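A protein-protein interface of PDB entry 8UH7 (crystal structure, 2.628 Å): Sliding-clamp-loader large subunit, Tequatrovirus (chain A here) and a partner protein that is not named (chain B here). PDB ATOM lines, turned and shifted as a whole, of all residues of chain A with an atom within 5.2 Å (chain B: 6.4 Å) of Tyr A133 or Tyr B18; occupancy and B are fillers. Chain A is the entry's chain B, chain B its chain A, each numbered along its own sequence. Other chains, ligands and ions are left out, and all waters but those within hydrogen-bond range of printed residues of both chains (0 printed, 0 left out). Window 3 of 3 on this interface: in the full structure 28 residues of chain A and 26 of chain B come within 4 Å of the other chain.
The side-chain hydroxyl of Tyr B18 is in hydrogen-bond range of the backbone carbonyl oxygen of Ala A132, at 2.7 Å. The backbone NH (N) of Phe A129 lies close to the indole nitrogen (NE1) of Trp B17 (3.5 Å).
The backbone carbonyl oxygen (O) of Tyr B18 lies within hydrogen-bond range of the side-chain amino group (NZ) of Lys B20, 3.3 Å away. The side-chain amide nitrogen (NE2) of Gln B14 sits at hydrogen-bond distance from the side-chain hydroxyl (OH) of Tyr B18, at 3.2 Å. The side-chain hydroxyl (OG) of Ser A98 sits at hydrogen-bond distance from the backbone carbonyl oxygen (O) of Thr A94 (2.5 Å). The backbone carbonyl oxygen (O) of Tyr A133 is in hydrogen-bond range of the side-chain sulfur (SG) of Cys A137 (3.5 Å).
Among the printed residues, pairs that only touch across the chains: Thr A94 with Trp B17 (3.3 Å), Glu A131 with His B13 (3.0 Å), Glu A131 with Gln B14 (3.9 Å), Ala A132 with Gln B14 (3.8 Å), Ala A132 with Trp B17 (3.9 Å), Tyr A133 with Trp B17 (3.7 Å) and Tyr A133 with Tyr B18 (3.7 Å).
Of chain B, only Trp B17 and Tyr B18 come within 4 Å of Tyr A133. Tyr B18 touches just these residues of chain A: Ala A132 (2.7 Å) and Tyr A133 (3.7 Å). Of the printed residues of chain B, Thr A94 touches Trp B17 (3.3 Å). Of the printed residues of chain A, His B13 touches Glu A131. The nearest residue of chain A that does not touch Tyr B18 is Asn A136 (4.8 Å). The nearest printed residue of chain A that does not touch Gln B14 is Ser A135 (5.8 Å).
Hydrophobic or aromatic side chains of chain A within 4 Å of the printed part of chain B: Phe A129, Ala A132 and Tyr A133. Printed residues of chain B that touch a printed residue of chain A: His B13, Gln B14, Trp B17 and Tyr B18. Hydrophobic or aromatic side chains of chain B within 4 Å of the printed part of chain A: His B13, Trp B17 and Tyr B18. Among the printed residues, 9 pairs touch across the chains. Among the printed residues, no Asp or Glu carboxylate lies within 4 Å of a Lys or Arg side-chain nitrogen of the other chain.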
ATOM      1  N   THR A  94       5.135  -6.963 -11.568  1.00  0.00           N
ATOM      2  CA  THR A  94       4.157  -6.442 -12.517  1.00  0.00           C
ATOM      3  C   THR A  94       3.232  -7.549 -13.011  1.00  0.00           C
ATOM      4  O   THR A  94       2.026  -7.331 -13.171  1.00  0.00           O
ATOM      5  CB  THR A  94       4.868  -5.768 -13.688  1.00  0.00           C
ATOM      6  OG1 THR A  94       5.919  -4.931 -13.191  1.00  0.00           O
ATOM      7  CG2 THR A  94       3.893  -4.913 -14.483  1.00  0.00           C
ATOM      8  N   ALA A  97       0.773  -8.084 -10.194  1.00  0.00           N
ATOM      9  CA  ALA A  97      -0.142  -6.970  -9.971  1.00  0.00           C
ATOM     10  C   ALA A  97      -1.175  -6.867 -11.084  1.00  0.00           C
ATOM     11  O   ALA A  97      -2.348  -6.577 -10.824  1.00  0.00           O
ATOM     12  CB  ALA A  97       0.641  -5.664  -9.850  1.00  0.00           C
ATOM     13  N   SER A  98      -0.760  -7.103 -12.329  1.00  0.00           N
ATOM     14  CA  SER A  98      -1.654  -6.937 -13.467  1.00  0.00           C
ATOM     15  C   SER A  98      -2.517  -8.164 -13.741  1.00  0.00           C
ATOM     16  O   SER A  98      -3.393  -8.099 -14.611  1.00  0.00           O
ATOM     17  CB  SER A  98      -0.843  -6.587 -14.715  1.00  0.00           C
ATOM     18  OG  SER A  98       0.230  -7.493 -14.890  1.00  0.00           O
ATOM     19  N   PHE A 129       6.360   1.789  -8.691  1.00  0.00           N
ATOM     20  CA  PHE A 129       5.397   0.699  -8.799  1.00  0.00           C
ATOM     21  C   PHE A 129       4.183   0.959  -7.915  1.00  0.00           C
ATOM     22  O   PHE A 129       3.038   0.790  -8.352  1.00  0.00           O
ATOM     23  CB  PHE A 129       6.088  -0.618  -8.428  1.00  0.00           C
ATOM     24  CG  PHE A 129       5.193  -1.825  -8.473  1.00  0.00           C
ATOM     25  CD1 PHE A 129       4.493  -2.228  -7.346  1.00  0.00           C
ATOM     26  CD2 PHE A 129       5.081  -2.578  -9.629  1.00  0.00           C
ATOM     27  CE1 PHE A 129       3.679  -3.341  -7.380  1.00  0.00           C
ATOM     28  CE2 PHE A 129       4.268  -3.697  -9.669  1.00  0.00           C
ATOM     29  CZ  PHE A 129       3.568  -4.078  -8.541  1.00  0.00           C
ATOM     30  N   MET A 130       4.416   1.418  -6.682  1.00  0.00           N
ATOM     31  CA  MET A 130       3.315   1.639  -5.752  1.00  0.00           C
ATOM     32  C   MET A 130       2.356   2.715  -6.237  1.00  0.00           C
ATOM     33  O   MET A 130       1.191   2.720  -5.830  1.00  0.00           O
ATOM     34  CB  MET A 130       3.855   2.011  -4.372  1.00  0.00           C
ATOM     35  CG  MET A 130       4.791   0.984  -3.776  1.00  0.00           C
ATOM     36  SD  MET A 130       5.336   1.444  -2.125  1.00  0.00           S
ATOM     37  CE  MET A 130       3.787   1.352  -1.243  1.00  0.00           C
ATOM     38  N   GLU A 131       2.812   3.626  -7.093  1.00  0.00           N
ATOM     39  CA  GLU A 131       1.944   4.668  -7.619  1.00  0.00           C
ATOM     40  C   GLU A 131       1.168   4.222  -8.848  1.00  0.00           C
ATOM     41  O   GLU A 131       0.324   4.979  -9.339  1.00  0.00           O
ATOM     42  CB  GLU A 131       2.762   5.923  -7.943  1.00  0.00           C
ATOM     43  CG  GLU A 131       3.228   6.679  -6.709  1.00  0.00           C
ATOM     44  CD  GLU A 131       2.609   8.060  -6.600  1.00  0.00           C
ATOM     45  OE1 GLU A 131       2.641   8.808  -7.601  1.00  0.00           O
ATOM     46  OE2 GLU A 131       2.085   8.396  -5.517  1.00  0.00           O
ATOM     47  N   ALA A 132       1.423   3.015  -9.352  1.00  0.00           N
ATOM     48  CA  ALA A 132       0.710   2.505 -10.515  1.00  0.00           C
ATOM     49  C   ALA A 132      -0.190   1.321 -10.208  1.00  0.00           C
ATOM     50  O   ALA A 132      -1.236   1.179 -10.843  1.00  0.00           O
ATOM     51  CB  ALA A 132       1.700   2.103 -11.614  1.00  0.00           C
ATOM     52  N   TYR A 133       0.178   0.478  -9.244  1.00  0.00           N
ATOM     53  CA  TYR A 133      -0.571  -0.735  -8.943  1.00  0.00           C
ATOM     54  C   TYR A 133      -1.042  -0.764  -7.492  1.00  0.00           C
ATOM     55  O   TYR A 133      -1.243  -1.838  -6.921  1.00  0.00           O
ATOM     56  CB  TYR A 133       0.265  -1.972  -9.264  1.00  0.00           C
ATOM     57  CG  TYR A 133       0.761  -2.021 -10.694  1.00  0.00           C
ATOM     58  CD1 TYR A 133       1.985  -1.469 -11.043  1.00  0.00           C
ATOM     59  CD2 TYR A 133       0.004  -2.619 -11.694  1.00  0.00           C
ATOM     60  CE1 TYR A 133       2.444  -1.511 -12.346  1.00  0.00           C
ATOM     61  CE2 TYR A 133       0.454  -2.665 -13.000  1.00  0.00           C
ATOM     62  CZ  TYR A 133       1.675  -2.110 -13.322  1.00  0.00           C
ATOM     63  OH  TYR A 133       2.132  -2.152 -14.621  1.00  0.00           O
ATOM     64  N   SER A 134      -1.224   0.411  -6.883  1.00  0.00           N
ATOM     65  CA  SER A 134      -1.736   0.458  -5.518  1.00  0.00           C
ATOM     66  C   SER A 134      -3.188   0.008  -5.449  1.00  0.00           C
ATOM     67  O   SER A 134      -3.598  -0.615  -4.462  1.00  0.00           O
ATOM     68  CB  SER A 134      -1.596   1.868  -4.949  1.00  0.00           C
ATOM     69  OG  SER A 134      -2.110   2.831  -5.852  1.00  0.00           O
ATOM     70  N   SER A 135      -3.979   0.313  -6.479  1.00  0.00           N
ATOM     71  CA  SER A 135      -5.365  -0.130  -6.527  1.00  0.00           C
ATOM     72  C   SER A 135      -5.499  -1.626  -6.781  1.00  0.00           C
ATOM     73  O   SER A 135      -6.601  -2.163  -6.627  1.00  0.00           O
ATOM     74  CB  SER A 135      -6.118   0.653  -7.605  1.00  0.00           C
ATOM     75  OG  SER A 135      -5.407   0.645  -8.831  1.00  0.00           O
ATOM     76  N   ASN A 136      -4.415  -2.307  -7.155  1.00  0.00           N
ATOM     77  CA  ASN A 136      -4.452  -3.736  -7.440  1.00  0.00           C
ATOM     78  C   ASN A 136      -3.869  -4.594  -6.326  1.00  0.00           C
ATOM     79  O   ASN A 136      -4.309  -5.736  -6.148  1.00  0.00           O
ATOM     80  CB  ASN A 136      -3.699  -4.036  -8.740  1.00  0.00           C
ATOM     81  CG  ASN A 136      -4.311  -3.345  -9.937  1.00  0.00           C
ATOM     82  OD1 ASN A 136      -5.178  -3.901 -10.612  1.00  0.00           O
ATOM     83  ND2 ASN A 136      -3.866  -2.124 -10.208  1.00  0.00           N
ATOM     84  N   CYS A 137      -2.898  -4.081  -5.576  1.00  0.00           N
ATOM     85  CA  CYS A 137      -2.231  -4.890  -4.567  1.00  0.00           C
ATOM     86  C   CYS A 137      -1.572  -3.984  -3.539  1.00  0.00           C
ATOM     87  O   CYS A 137      -1.384  -2.786  -3.766  1.00  0.00           O
ATOM     88  CB  CYS A 137      -1.190  -5.817  -5.199  1.00  0.00           C
ATOM     89  SG  CYS A 137       0.128  -4.933  -6.055  1.00  0.00           S
ATOM     90  N   LEU B  10      -4.081   9.445 -16.396  1.00  0.00           N
ATOM     91  CA  LEU B  10      -3.257   8.795 -15.393  1.00  0.00           C
ATOM     92  C   LEU B  10      -2.073   9.678 -15.017  1.00  0.00           C
ATOM     93  O   LEU B  10      -1.699  10.603 -15.741  1.00  0.00           O
ATOM     94  CB  LEU B  10      -2.756   7.450 -15.918  1.00  0.00           C
ATOM     95  CG  LEU B  10      -3.769   6.605 -16.692  1.00  0.00           C
ATOM     96  CD1 LEU B  10      -3.108   5.368 -17.276  1.00  0.00           C
ATOM     97  CD2 LEU B  10      -4.935   6.221 -15.797  1.00  0.00           C
ATOM     98  N   HIS B  13       3.531   7.858 -13.394  1.00  0.00           N
ATOM     99  CA  HIS B  13       3.935   6.499 -13.046  1.00  0.00           C
ATOM    100  C   HIS B  13       3.081   5.463 -13.767  1.00  0.00           C
ATOM    101  O   HIS B  13       3.607   4.467 -14.279  1.00  0.00           O
ATOM    102  CB  HIS B  13       3.855   6.303 -11.533  1.00  0.00           C
ATOM    103  CG  HIS B  13       4.720   7.244 -10.755  1.00  0.00           C
ATOM    104  ND1 HIS B  13       6.092   7.120 -10.700  1.00  0.00           N
ATOM    105  CD2 HIS B  13       4.409   8.325 -10.000  1.00  0.00           C
ATOM    106  CE1 HIS B  13       6.588   8.084  -9.946  1.00  0.00           C
ATOM    107  NE2 HIS B  13       5.589   8.829  -9.508  1.00  0.00           N
ATOM    108  N   GLN B  14       1.763   5.674 -13.811  1.00  0.00           N
ATOM    109  CA  GLN B  14       0.890   4.747 -14.525  1.00  0.00           C
ATOM    110  C   GLN B  14       1.214   4.720 -16.012  1.00  0.00           C
ATOM    111  O   GLN B  14       1.250   3.649 -16.629  1.00  0.00           O
ATOM    112  CB  GLN B  14      -0.573   5.125 -14.307  1.00  0.00           C
ATOM    113  CG  GLN B  14      -1.108   4.800 -12.930  1.00  0.00           C
ATOM    114  CD  GLN B  14      -2.537   5.268 -12.745  1.00  0.00           C
ATOM    115  OE1 GLN B  14      -2.794   6.457 -12.557  1.00  0.00           O
ATOM    116  NE2 GLN B  14      -3.477   4.331 -12.805  1.00  0.00           N
ATOM    117  N   VAL B  15       1.447   5.891 -16.610  1.00  0.00           N
ATOM    118  CA  VAL B  15       1.781   5.940 -18.029  1.00  0.00           C
ATOM    119  C   VAL B  15       3.098   5.223 -18.288  1.00  0.00           C
ATOM    120  O   VAL B  15       3.257   4.531 -19.300  1.00  0.00           O
ATOM    121  CB  VAL B  15       1.821   7.400 -18.520  1.00  0.00           C
ATOM    122  CG1 VAL B  15       2.191   7.460 -19.996  1.00  0.00           C
ATOM    123  CG2 VAL B  15       0.482   8.076 -18.277  1.00  0.00           C
ATOM    124  N   ALA B  16       4.057   5.361 -17.369  1.00  0.00           N
ATOM    125  CA  ALA B  16       5.353   4.715 -17.553  1.00  0.00           C
ATOM    126  C   ALA B  16       5.244   3.201 -17.422  1.00  0.00           C
ATOM    127  O   ALA B  16       5.847   2.459 -18.207  1.00  0.00           O
ATOM    128  CB  ALA B  16       6.362   5.268 -16.549  1.00  0.00           C
ATOM    129  N   TRP B  17       4.477   2.723 -16.442  1.00  0.00           N
ATOM    130  CA  TRP B  17       4.419   1.289 -16.177  1.00  0.00           C
ATOM    131  C   TRP B  17       3.519   0.562 -17.173  1.00  0.00           C
ATOM    132  O   TRP B  17       3.915  -0.460 -17.742  1.00  0.00           O
ATOM    133  CB  TRP B  17       3.953   1.039 -14.741  1.00  0.00           C
ATOM    134  CG  TRP B  17       5.054   1.172 -13.727  1.00  0.00           C
ATOM    135  CD1 TRP B  17       5.359   2.276 -12.984  1.00  0.00           C
ATOM    136  CD2 TRP B  17       5.999   0.164 -13.351  1.00  0.00           C
ATOM    137  NE1 TRP B  17       6.434   2.017 -12.166  1.00  0.00           N
ATOM    138  CE2 TRP B  17       6.845   0.727 -12.373  1.00  0.00           C
ATOM    139  CE3 TRP B  17       6.211  -1.161 -13.745  1.00  0.00           C
ATOM    140  CZ2 TRP B  17       7.886   0.010 -11.785  1.00  0.00           C
ATOM    141  CZ3 TRP B  17       7.247  -1.870 -13.161  1.00  0.00           C
ATOM    142  CH2 TRP B  17       8.070  -1.283 -12.191  1.00  0.00           C
ATOM    143  N   TYR B  18       2.306   1.073 -17.395  1.00  0.00           N
ATOM    144  CA  TYR B  18       1.374   0.400 -18.296  1.00  0.00           C
ATOM    145  C   TYR B  18       1.927   0.331 -19.715  1.00  0.00           C
ATOM    146  O   TYR B  18       1.705  -0.655 -20.428  1.00  0.00           O
ATOM    147  CB  TYR B  18       0.022   1.111 -18.283  1.00  0.00           C
ATOM    148  CG  TYR B  18      -0.643   1.157 -16.927  1.00  0.00           C
ATOM    149  CD1 TYR B  18      -0.365   0.199 -15.959  1.00  0.00           C
ATOM    150  CD2 TYR B  18      -1.551   2.158 -16.614  1.00  0.00           C
ATOM    151  CE1 TYR B  18      -0.975   0.241 -14.717  1.00  0.00           C
ATOM    152  CE2 TYR B  18      -2.164   2.208 -15.377  1.00  0.00           C
ATOM    153  CZ  TYR B  18      -1.872   1.249 -14.433  1.00  0.00           C
ATOM    154  OH  TYR B  18      -2.483   1.302 -13.204  1.00  0.00           O
ATOM    155  N   SER B  19       2.647   1.370 -20.144  1.00  0.00           N
ATOM    156  CA  SER B  19       3.297   1.347 -21.448  1.00  0.00           C
ATOM    157  C   SER B  19       4.532   0.462 -21.466  1.00  0.00           C
ATOM    158  O   SER B  19       4.994   0.090 -22.551  1.00  0.00           O
ATOM    159  CB  SER B  19       3.683   2.764 -21.877  1.00  0.00           C
ATOM    160  OG  SER B  19       4.538   3.374 -20.927  1.00  0.00           O
ATOM    161  N   LYS B  20       5.070   0.122 -20.294  1.00  0.00           N
ATOM    162  CA  LYS B  20       6.277  -0.692 -20.173  1.00  0.00           C
ATOM    163  C   LYS B  20       7.463  -0.057 -20.894  1.00  0.00           C
ATOM    164  O   LYS B  20       8.350  -0.755 -21.391  1.00  0.00           O
ATOM    165  CB  LYS B  20       6.038  -2.119 -20.674  1.00  0.00           C
ATOM    166  CG  LYS B  20       4.900  -2.825 -19.961  1.00  0.00           C
ATOM    167  CD  LYS B  20       4.653  -4.199 -20.552  1.00  0.00           C
ATOM    168  CE  LYS B  20       3.362  -4.798 -20.025  1.00  0.00           C
ATOM    169  NZ  LYS B  20       2.176  -3.933 -20.293  1.00  0.00           N
ATOM    170  N   ASP B  21       7.482   1.272 -20.961  1.00  0.00           N
ATOM    171  CA  ASP B  21       8.646   2.012 -21.443  1.00  0.00           C
ATOM    172  C   ASP B  21       9.574   2.203 -20.252  1.00  0.00           C
ATOM    173  O   ASP B  21       9.362   3.088 -19.419  1.00  0.00           O
ATOM    174  CB  ASP B  21       8.237   3.343 -22.058  1.00  0.00           C
ATOM    175  CG  ASP B  21       9.426   4.144 -22.542  1.00  0.00           C
ATOM    176  OD1 ASP B  21      10.038   3.748 -23.557  1.00  0.00           O
ATOM    177  OD2 ASP B  21       9.754   5.163 -21.901  1.00  0.00           O
